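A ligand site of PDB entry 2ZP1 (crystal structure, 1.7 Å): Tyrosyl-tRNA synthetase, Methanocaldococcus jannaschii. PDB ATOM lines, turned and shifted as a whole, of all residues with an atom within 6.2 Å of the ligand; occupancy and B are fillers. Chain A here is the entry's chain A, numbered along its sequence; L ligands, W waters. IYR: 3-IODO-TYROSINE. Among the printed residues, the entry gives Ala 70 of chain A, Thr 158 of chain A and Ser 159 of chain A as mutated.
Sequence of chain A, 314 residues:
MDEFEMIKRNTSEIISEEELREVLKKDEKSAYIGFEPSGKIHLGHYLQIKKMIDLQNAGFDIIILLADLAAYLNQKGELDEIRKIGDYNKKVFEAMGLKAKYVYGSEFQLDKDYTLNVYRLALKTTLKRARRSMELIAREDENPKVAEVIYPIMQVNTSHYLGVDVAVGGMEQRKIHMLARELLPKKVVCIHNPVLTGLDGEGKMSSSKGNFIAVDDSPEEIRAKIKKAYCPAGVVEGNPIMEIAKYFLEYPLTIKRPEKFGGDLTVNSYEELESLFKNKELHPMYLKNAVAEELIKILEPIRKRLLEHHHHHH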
ATOM      1  N   TYR A  32      12.522 -11.550   7.454  1.00  0.00           N
ATOM      2  CA  TYR A  32      13.903 -11.600   7.933  1.00  0.00           C
ATOM      3  C   TYR A  32      14.779 -10.672   7.133  1.00  0.00           C
ATOM      4  O   TYR A  32      14.392 -10.178   6.058  1.00  0.00           O
ATOM      5  CB  TYR A  32      14.508 -13.037   7.858  1.00  0.00           C
ATOM      6  CG  TYR A  32      15.408 -13.325   6.663  1.00  0.00           C
ATOM      7  CD1 TYR A  32      16.796 -13.480   6.828  1.00  0.00           C
ATOM      8  CD2 TYR A  32      14.877 -13.479   5.390  1.00  0.00           C
ATOM      9  CE1 TYR A  32      17.636 -13.786   5.734  1.00  0.00           C
ATOM     10  CE2 TYR A  32      15.699 -13.775   4.287  1.00  0.00           C
ATOM     11  CZ  TYR A  32      17.063 -13.920   4.477  1.00  0.00           C
ATOM     12  OH  TYR A  32      17.845 -14.218   3.384  1.00  0.00           O
ATOM     13  N   ILE A  33      15.947 -10.405   7.715  1.00  0.00           N
ATOM     14  CA  ILE A  33      16.999  -9.652   7.032  1.00  0.00           C
ATOM     15  C   ILE A  33      18.274 -10.289   7.559  1.00  0.00           C
ATOM     16  O   ILE A  33      18.320 -10.748   8.718  1.00  0.00           O
ATOM     17  CB  ILE A  33      16.994  -8.137   7.326  1.00  0.00           C
ATOM     18  CG1 ILE A  33      18.189  -7.481   6.610  1.00  0.00           C
ATOM     19  CG2 ILE A  33      17.008  -7.850   8.855  1.00  0.00           C
ATOM     20  CD1 ILE A  33      18.020  -5.966   6.499  1.00  0.00           C
ATOM     21  N   GLY A  34      19.291 -10.388   6.711  1.00  0.00           N
ATOM     22  CA  GLY A  34      20.538 -10.940   7.196  1.00  0.00           C
ATOM     23  C   GLY A  34      21.644  -9.898   7.058  1.00  0.00           C
ATOM     24  O   GLY A  34      21.589  -9.052   6.173  1.00  0.00           O
ATOM     25  N   PHE A  35      22.621  -9.938   7.968  1.00  0.00           N
ATOM     26  CA  PHE A  35      23.755  -9.017   7.901  1.00  0.00           C
ATOM     27  C   PHE A  35      25.045  -9.786   8.116  1.00  0.00           C
ATOM     28  O   PHE A  35      25.119 -10.596   9.033  1.00  0.00           O
ATOM     29  CB  PHE A  35      23.749  -7.978   9.018  1.00  0.00           C
ATOM     30  CG  PHE A  35      22.552  -7.077   9.029  1.00  0.00           C
ATOM     31  CD1 PHE A  35      21.522  -7.298   9.955  1.00  0.00           C
ATOM     32  CD2 PHE A  35      22.487  -5.997   8.186  1.00  0.00           C
ATOM     33  CE1 PHE A  35      20.458  -6.431  10.038  1.00  0.00           C
ATOM     34  CE2 PHE A  35      21.419  -5.111   8.244  1.00  0.00           C
ATOM     35  CZ  PHE A  35      20.407  -5.334   9.186  1.00  0.00           C
ATOM     36  N   GLU A  36      26.037  -9.548   7.259  1.00  0.00           N
ATOM     37  CA  GLU A  36      27.361 -10.101   7.530  1.00  0.00           C
ATOM     38  C   GLU A  36      27.789  -9.295   8.774  1.00  0.00           C
ATOM     39  O   GLU A  36      27.702  -8.060   8.770  1.00  0.00           O
ATOM     40  CB  GLU A  36      28.304  -9.784   6.375  1.00  0.00           C
ATOM     41  CG  GLU A  36      28.051 -10.604   5.133  1.00  0.00           C
ATOM     42  CD  GLU A  36      29.130 -10.378   4.074  1.00  0.00           C
ATOM     43  OE1 GLU A  36      30.295 -10.181   4.481  1.00  0.00           O
ATOM     44  OE2 GLU A  36      28.812 -10.415   2.873  1.00  0.00           O
ATOM     45  N   LEU A  65      19.127 -12.647  10.769  1.00  0.00           N
ATOM     46  CA  LEU A  65      20.162 -13.627  10.506  1.00  0.00           C
ATOM     47  C   LEU A  65      21.519 -12.965  10.659  1.00  0.00           C
ATOM     48  O   LEU A  65      21.806 -11.983   9.981  1.00  0.00           O
ATOM     49  CB  LEU A  65      20.026 -14.201   9.082  1.00  0.00           C
ATOM     50  CG  LEU A  65      21.185 -15.108   8.665  1.00  0.00           C
ATOM     51  CD1 LEU A  65      20.998 -16.461   9.331  1.00  0.00           C
ATOM     52  CD2 LEU A  65      21.239 -15.282   7.140  1.00  0.00           C
ATOM     53  N   ALA A  67      24.641 -13.386   9.627  1.00  0.00           N
ATOM     54  CA  ALA A  67      25.138 -14.190   8.508  1.00  0.00           C
ATOM     55  C   ALA A  67      26.617 -14.532   8.586  1.00  0.00           C
ATOM     56  O   ALA A  67      27.420 -14.062   7.774  1.00  0.00           O
ATOM     57  CB  ALA A  67      24.822 -13.466   7.196  1.00  0.00           C
ATOM     58  N   ALA A  70      28.048 -16.654   5.543  1.00  0.00           N
ATOM     59  CA  ALA A  70      28.146 -15.810   4.345  1.00  0.00           C
ATOM     60  C   ALA A  70      29.370 -14.920   4.471  1.00  0.00           C
ATOM     61  O   ALA A  70      30.154 -14.770   3.519  1.00  0.00           O
ATOM     62  CB  ALA A  70      26.896 -14.960   4.201  1.00  0.00           C
ATOM     63  N   GLN A 109      22.894 -23.688   8.136  1.00  0.00           N
ATOM     64  CA  GLN A 109      23.327 -23.699   6.741  1.00  0.00           C
ATOM     65  C   GLN A 109      24.364 -24.738   6.339  1.00  0.00           C
ATOM     66  O   GLN A 109      24.807 -24.768   5.187  1.00  0.00           O
ATOM     67  CB  GLN A 109      23.776 -22.292   6.356  1.00  0.00           C
ATOM     68  CG  GLN A 109      22.583 -21.324   6.361  1.00  0.00           C
ATOM     69  CD  GLN A 109      22.986 -19.879   6.202  1.00  0.00           C
ATOM     70  OE1 GLN A 109      22.225 -19.076   5.642  1.00  0.00           O
ATOM     71  NE2 GLN A 109      24.148 -19.531   6.694  1.00  0.00           N
ATOM     72  N   TYR A 114      20.189 -28.765   3.890  1.00  0.00           N
ATOM     73  CA  TYR A 114      20.392 -27.398   3.402  1.00  0.00           C
ATOM     74  C   TYR A 114      21.365 -27.470   2.223  1.00  0.00           C
ATOM     75  O   TYR A 114      21.123 -26.902   1.156  1.00  0.00           O
ATOM     76  CB  TYR A 114      21.035 -26.526   4.468  1.00  0.00           C
ATOM     77  CG  TYR A 114      20.931 -25.049   4.193  1.00  0.00           C
ATOM     78  CD1 TYR A 114      19.903 -24.297   4.759  1.00  0.00           C
ATOM     79  CD2 TYR A 114      21.835 -24.402   3.343  1.00  0.00           C
ATOM     80  CE1 TYR A 114      19.771 -22.944   4.487  1.00  0.00           C
ATOM     81  CE2 TYR A 114      21.705 -23.019   3.065  1.00  0.00           C
ATOM     82  CZ  TYR A 114      20.661 -22.315   3.646  1.00  0.00           C
ATOM     83  OH  TYR A 114      20.465 -20.978   3.375  1.00  0.00           O
ATOM     84  N   ILE A 137      28.258  -6.762  -3.517  1.00  0.00           N
ATOM     85  CA  ILE A 137      28.389  -7.418  -2.228  1.00  0.00           C
ATOM     86  C   ILE A 137      29.761  -8.049  -2.012  1.00  0.00           C
ATOM     87  O   ILE A 137      30.347  -7.980  -0.922  1.00  0.00           O
ATOM     88  CB  ILE A 137      27.291  -8.503  -2.117  1.00  0.00           C
ATOM     89  CG1 ILE A 137      25.904  -7.846  -2.095  1.00  0.00           C
ATOM     90  CG2 ILE A 137      27.485  -9.335  -0.873  1.00  0.00           C
ATOM     91  CD1 ILE A 137      24.797  -8.823  -2.463  1.00  0.00           C
ATOM     92  N   TYR A 151      28.071 -18.130  -2.265  1.00  0.00           N
ATOM     93  CA  TYR A 151      27.393 -17.149  -1.433  1.00  0.00           C
ATOM     94  C   TYR A 151      25.945 -16.836  -1.881  1.00  0.00           C
ATOM     95  O   TYR A 151      24.994 -17.031  -1.105  1.00  0.00           O
ATOM     96  CB  TYR A 151      28.235 -15.872  -1.400  1.00  0.00           C
ATOM     97  CG  TYR A 151      27.762 -14.789  -0.474  1.00  0.00           C
ATOM     98  CD1 TYR A 151      28.558 -14.382   0.597  1.00  0.00           C
ATOM     99  CD2 TYR A 151      26.582 -14.082  -0.726  1.00  0.00           C
ATOM    100  CE1 TYR A 151      28.202 -13.284   1.397  1.00  0.00           C
ATOM    101  CE2 TYR A 151      26.220 -12.986   0.061  1.00  0.00           C
ATOM    102  CZ  TYR A 151      27.027 -12.585   1.104  1.00  0.00           C
ATOM    103  OH  TYR A 151      26.699 -11.455   1.838  1.00  0.00           O
ATOM    104  N   MET A 154      23.535 -19.753  -1.393  1.00  0.00           N
ATOM    105  CA  MET A 154      23.311 -20.024   0.019  1.00  0.00           C
ATOM    106  C   MET A 154      22.261 -19.005   0.502  1.00  0.00           C
ATOM    107  O   MET A 154      21.365 -19.355   1.272  1.00  0.00           O
ATOM    108  CB  MET A 154      24.581 -19.827   0.827  1.00  0.00           C
ATOM    109  CG  MET A 154      24.380 -20.065   2.325  1.00  0.00           C
ATOM    110  SD  MET A 154      25.941 -19.957   3.198  1.00  0.00           S
ATOM    111  CE  MET A 154      26.684 -21.504   2.656  1.00  0.00           C
ATOM    112  N   GLN A 155      22.395 -17.748   0.056  1.00  0.00           N
ATOM    113  CA  GLN A 155      21.416 -16.716   0.457  1.00  0.00           C
ATOM    114  C   GLN A 155      20.015 -16.991  -0.121  1.00  0.00           C
ATOM    115  O   GLN A 155      19.009 -16.754   0.557  1.00  0.00           O
ATOM    116  CB  GLN A 155      21.901 -15.317   0.025  1.00  0.00           C
ATOM    117  CG  GLN A 155      20.964 -14.219   0.497  1.00  0.00           C
ATOM    118  CD  GLN A 155      21.606 -12.854   0.417  1.00  0.00           C
ATOM    119  OE1 GLN A 155      22.828 -12.742   0.390  1.00  0.00           O
ATOM    120  NE2 GLN A 155      20.778 -11.802   0.393  1.00  0.00           N
ATOM    121  N   VAL A 156      19.938 -17.466  -1.354  1.00  0.00           N
ATOM    122  CA  VAL A 156      18.641 -17.795  -1.930  1.00  0.00           C
ATOM    123  C   VAL A 156      17.975 -18.863  -1.066  1.00  0.00           C
ATOM    124  O   VAL A 156      16.789 -18.758  -0.748  1.00  0.00           O
ATOM    125  CB  VAL A 156      18.768 -18.339  -3.360  1.00  0.00           C
ATOM    126  CG1 VAL A 156      17.432 -19.006  -3.796  1.00  0.00           C
ATOM    127  CG2 VAL A 156      19.125 -17.209  -4.315  1.00  0.00           C
ATOM    128  N   THR A 158      18.236 -19.413   2.140  1.00  0.00           N
ATOM    129  CA  THR A 158      17.798 -18.984   3.463  1.00  0.00           C
ATOM    130  C   THR A 158      16.306 -18.716   3.553  1.00  0.00           C
ATOM    131  O   THR A 158      15.669 -19.164   4.507  1.00  0.00           O
ATOM    132  CB  THR A 158      18.500 -17.696   3.911  1.00  0.00           C
ATOM    133  OG1 THR A 158      19.899 -17.914   3.838  1.00  0.00           O
ATOM    134  CG2 THR A 158      18.143 -17.362   5.379  1.00  0.00           C
ATOM    135  N   SER A 159      15.758 -17.979   2.587  1.00  0.00           N
ATOM    136  CA  SER A 159      14.322 -17.680   2.576  1.00  0.00           C
ATOM    137  C   SER A 159      13.533 -18.958   2.534  1.00  0.00           C
ATOM    138  O   SER A 159      12.531 -19.099   3.230  1.00  0.00           O
ATOM    139  CB  SER A 159      13.927 -16.877   1.325  1.00  0.00           C
ATOM    140  OG  SER A 159      14.448 -15.565   1.371  1.00  0.00           O
ATOM    141  N   GLN A 173      21.077  -6.079  -2.558  1.00  0.00           N
ATOM    142  CA  GLN A 173      20.601  -7.470  -2.524  1.00  0.00           C
ATOM    143  C   GLN A 173      19.585  -7.808  -3.594  1.00  0.00           C
ATOM    144  O   GLN A 173      19.190  -8.970  -3.731  1.00  0.00           O
ATOM    145  CB  GLN A 173      19.937  -7.777  -1.167  1.00  0.00           C
ATOM    146  CG  GLN A 173      20.708  -7.344   0.075  1.00  0.00           C
ATOM    147  CD  GLN A 173      22.092  -8.000   0.188  1.00  0.00           C
ATOM    148  OE1 GLN A 173      22.227  -9.217   0.042  1.00  0.00           O
ATOM    149  NE2 GLN A 173      23.097  -7.187   0.457  1.00  0.00           N
ATOM    150  N   ILE A 176      20.212 -10.923  -6.000  1.00  0.00           N
ATOM    151  CA  ILE A 176      20.085 -12.216  -5.323  1.00  0.00           C
ATOM    152  C   ILE A 176      18.598 -12.492  -5.077  1.00  0.00           C
ATOM    153  O   ILE A 176      18.134 -13.608  -5.262  1.00  0.00           O
ATOM    154  CB  ILE A 176      20.834 -12.221  -3.979  1.00  0.00           C
ATOM    155  CG1 ILE A 176      22.349 -12.260  -4.245  1.00  0.00           C
ATOM    156  CG2 ILE A 176      20.424 -13.451  -3.132  1.00  0.00           C
ATOM    157  CD1 ILE A 176      23.172 -12.092  -2.996  1.00  0.00           C
ATOM    158  N   HIS A 177      17.834 -11.477  -4.661  1.00  0.00           N
ATOM    159  CA  HIS A 177      16.395 -11.683  -4.401  1.00  0.00           C
ATOM    160  C   HIS A 177      15.623 -12.029  -5.674  1.00  0.00           C
ATOM    161  O   HIS A 177      14.706 -12.839  -5.645  1.00  0.00           O
ATOM    162  CB  HIS A 177      15.799 -10.440  -3.699  1.00  0.00           C
ATOM    163  CG  HIS A 177      16.153 -10.341  -2.235  1.00  0.00           C
ATOM    164  ND1 HIS A 177      16.066  -9.165  -1.522  1.00  0.00           N
ATOM    165  CD2 HIS A 177      16.596 -11.279  -1.367  1.00  0.00           C
ATOM    166  CE1 HIS A 177      16.431  -9.384  -0.274  1.00  0.00           C
ATOM    167  NE2 HIS A 177      16.755 -10.653  -0.150  1.00  0.00           N
HETATM  168  N   IYR L   1      24.071 -10.518   1.702  1.00  0.00           N
HETATM  169  CA  IYR L   1      23.895  -9.882   3.052  1.00  0.00           C
HETATM  170  CB  IYR L   1      24.082 -10.936   4.157  1.00  0.00           C
HETATM  171  CC  IYR L   1      23.060 -12.043   4.065  1.00  0.00           C
HETATM  172  CD  IYR L   1      23.468 -13.378   3.958  1.00  0.00           C
HETATM  173  CE  IYR L   1      22.539 -14.426   3.853  1.00  0.00           C
HETATM  174  IE  IYR L   1      23.187 -16.364   3.634  1.00  0.00           I
HETATM  175  CF  IYR L   1      21.169 -14.116   3.865  1.00  0.00           C
HETATM  176  OF  IYR L   1      20.215 -15.111   3.778  1.00  0.00           O
HETATM  177  CG  IYR L   1      20.738 -12.787   3.968  1.00  0.00           C
HETATM  178  CH  IYR L   1      21.684 -11.758   4.076  1.00  0.00           C
HETATM  179  C   IYR L   1      24.880  -8.726   3.254  1.00  0.00           C
HETATM  180  O   IYR L   1      25.333  -8.183   2.225  1.00  0.00           O
HETATM  181  OXT IYR L   1      25.162  -8.365   4.414  1.00  0.00           O
HETATM  182  O   HOH W   1      27.117  -6.332   2.103  1.00  0.00           O
HETATM  183  O   HOH W   2      18.175 -11.835   1.884  1.00  0.00           O
HETATM  184  O   HOH W   3      20.911  -8.244   3.675  1.00  0.00           O
HETATM  185  O   HOH W   4      25.516  -5.870   5.380  1.00  0.00           O
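The side-chain hydroxyl (OH) of Tyr 32 is in hydrogen-bond range of an oxygen (OF) of the ligand (2.6 Å). OE1 of Gln 173 is in hydrogen-bond range of N of the ligand (2.8 Å). The side-chain hydroxyl (OG1) of Thr 158 sits at hydrogen-bond distance from an oxygen (OF) of the ligand, 2.8 Å away. The side-chain amide oxygen (OE1) of Gln 155 lies within hydrogen-bond range of a nitrogen (N) of the ligand, at 2.9 Å. A nitrogen (N) of the ligand sits at hydrogen-bond distance from the side-chain hydroxyl (OH) of Tyr 151, 2.8 Å away. The backbone NH (N) of Glu 36 lies within hydrogen-bond range of an oxygen (OXT) of the ligand, at 3.2 Å.
Water W2 lies within hydrogen-bond range of a ring nitrogen (NE2) of His 177 (2.7 Å), the side-chain hydroxyl (OH) of Tyr 32 (2.8 Å) and the side-chain amide nitrogen (NE2) of Gln 155 (3.0 Å).
Residues that only touch the ligand: Gly 34 (3.4 Å), Leu 65 (3.5 Å), Gln 109 (3.5 Å), Ala 67 (3.5 Å), Ala 70 (3.8 Å), Phe 35 (3.8 Å) and Ile 137 (3.9 Å). The nearest printed residue that does not touch the ligand is Met 154 (4.1 Å).
N of Thr 158 sits at hydrogen-bond distance from OH of Tyr 114, 3.0 Å away. The side-chain amide oxygen (OE1) of Gln 109 lies within hydrogen-bond range of the side-chain hydroxyl (OG1) of Thr 158 (3.2 Å). The side-chain amide oxygen (OE1) of Gln 173 lies within hydrogen-bond range of the side-chain amide nitrogen (NE2) of Gln 155 (3.0 Å). N of Leu 65 sits at hydrogen-bond distance from O of Ile 33 (2.9 Å). The side-chain hydroxyl of Thr 158 lies within hydrogen-bond range of the backbone carbonyl oxygen of Met 154 (3.3 Å). OH of Tyr 151 sits at hydrogen-bond distance from OE2 of Glu 36 (2.6 Å). OE1 of Gln 109 lies within hydrogen-bond range of OH of Tyr 114. The backbone NH of Phe 35 sits at hydrogen-bond distance from the backbone carbonyl oxygen of Leu 65 (3.0 Å).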
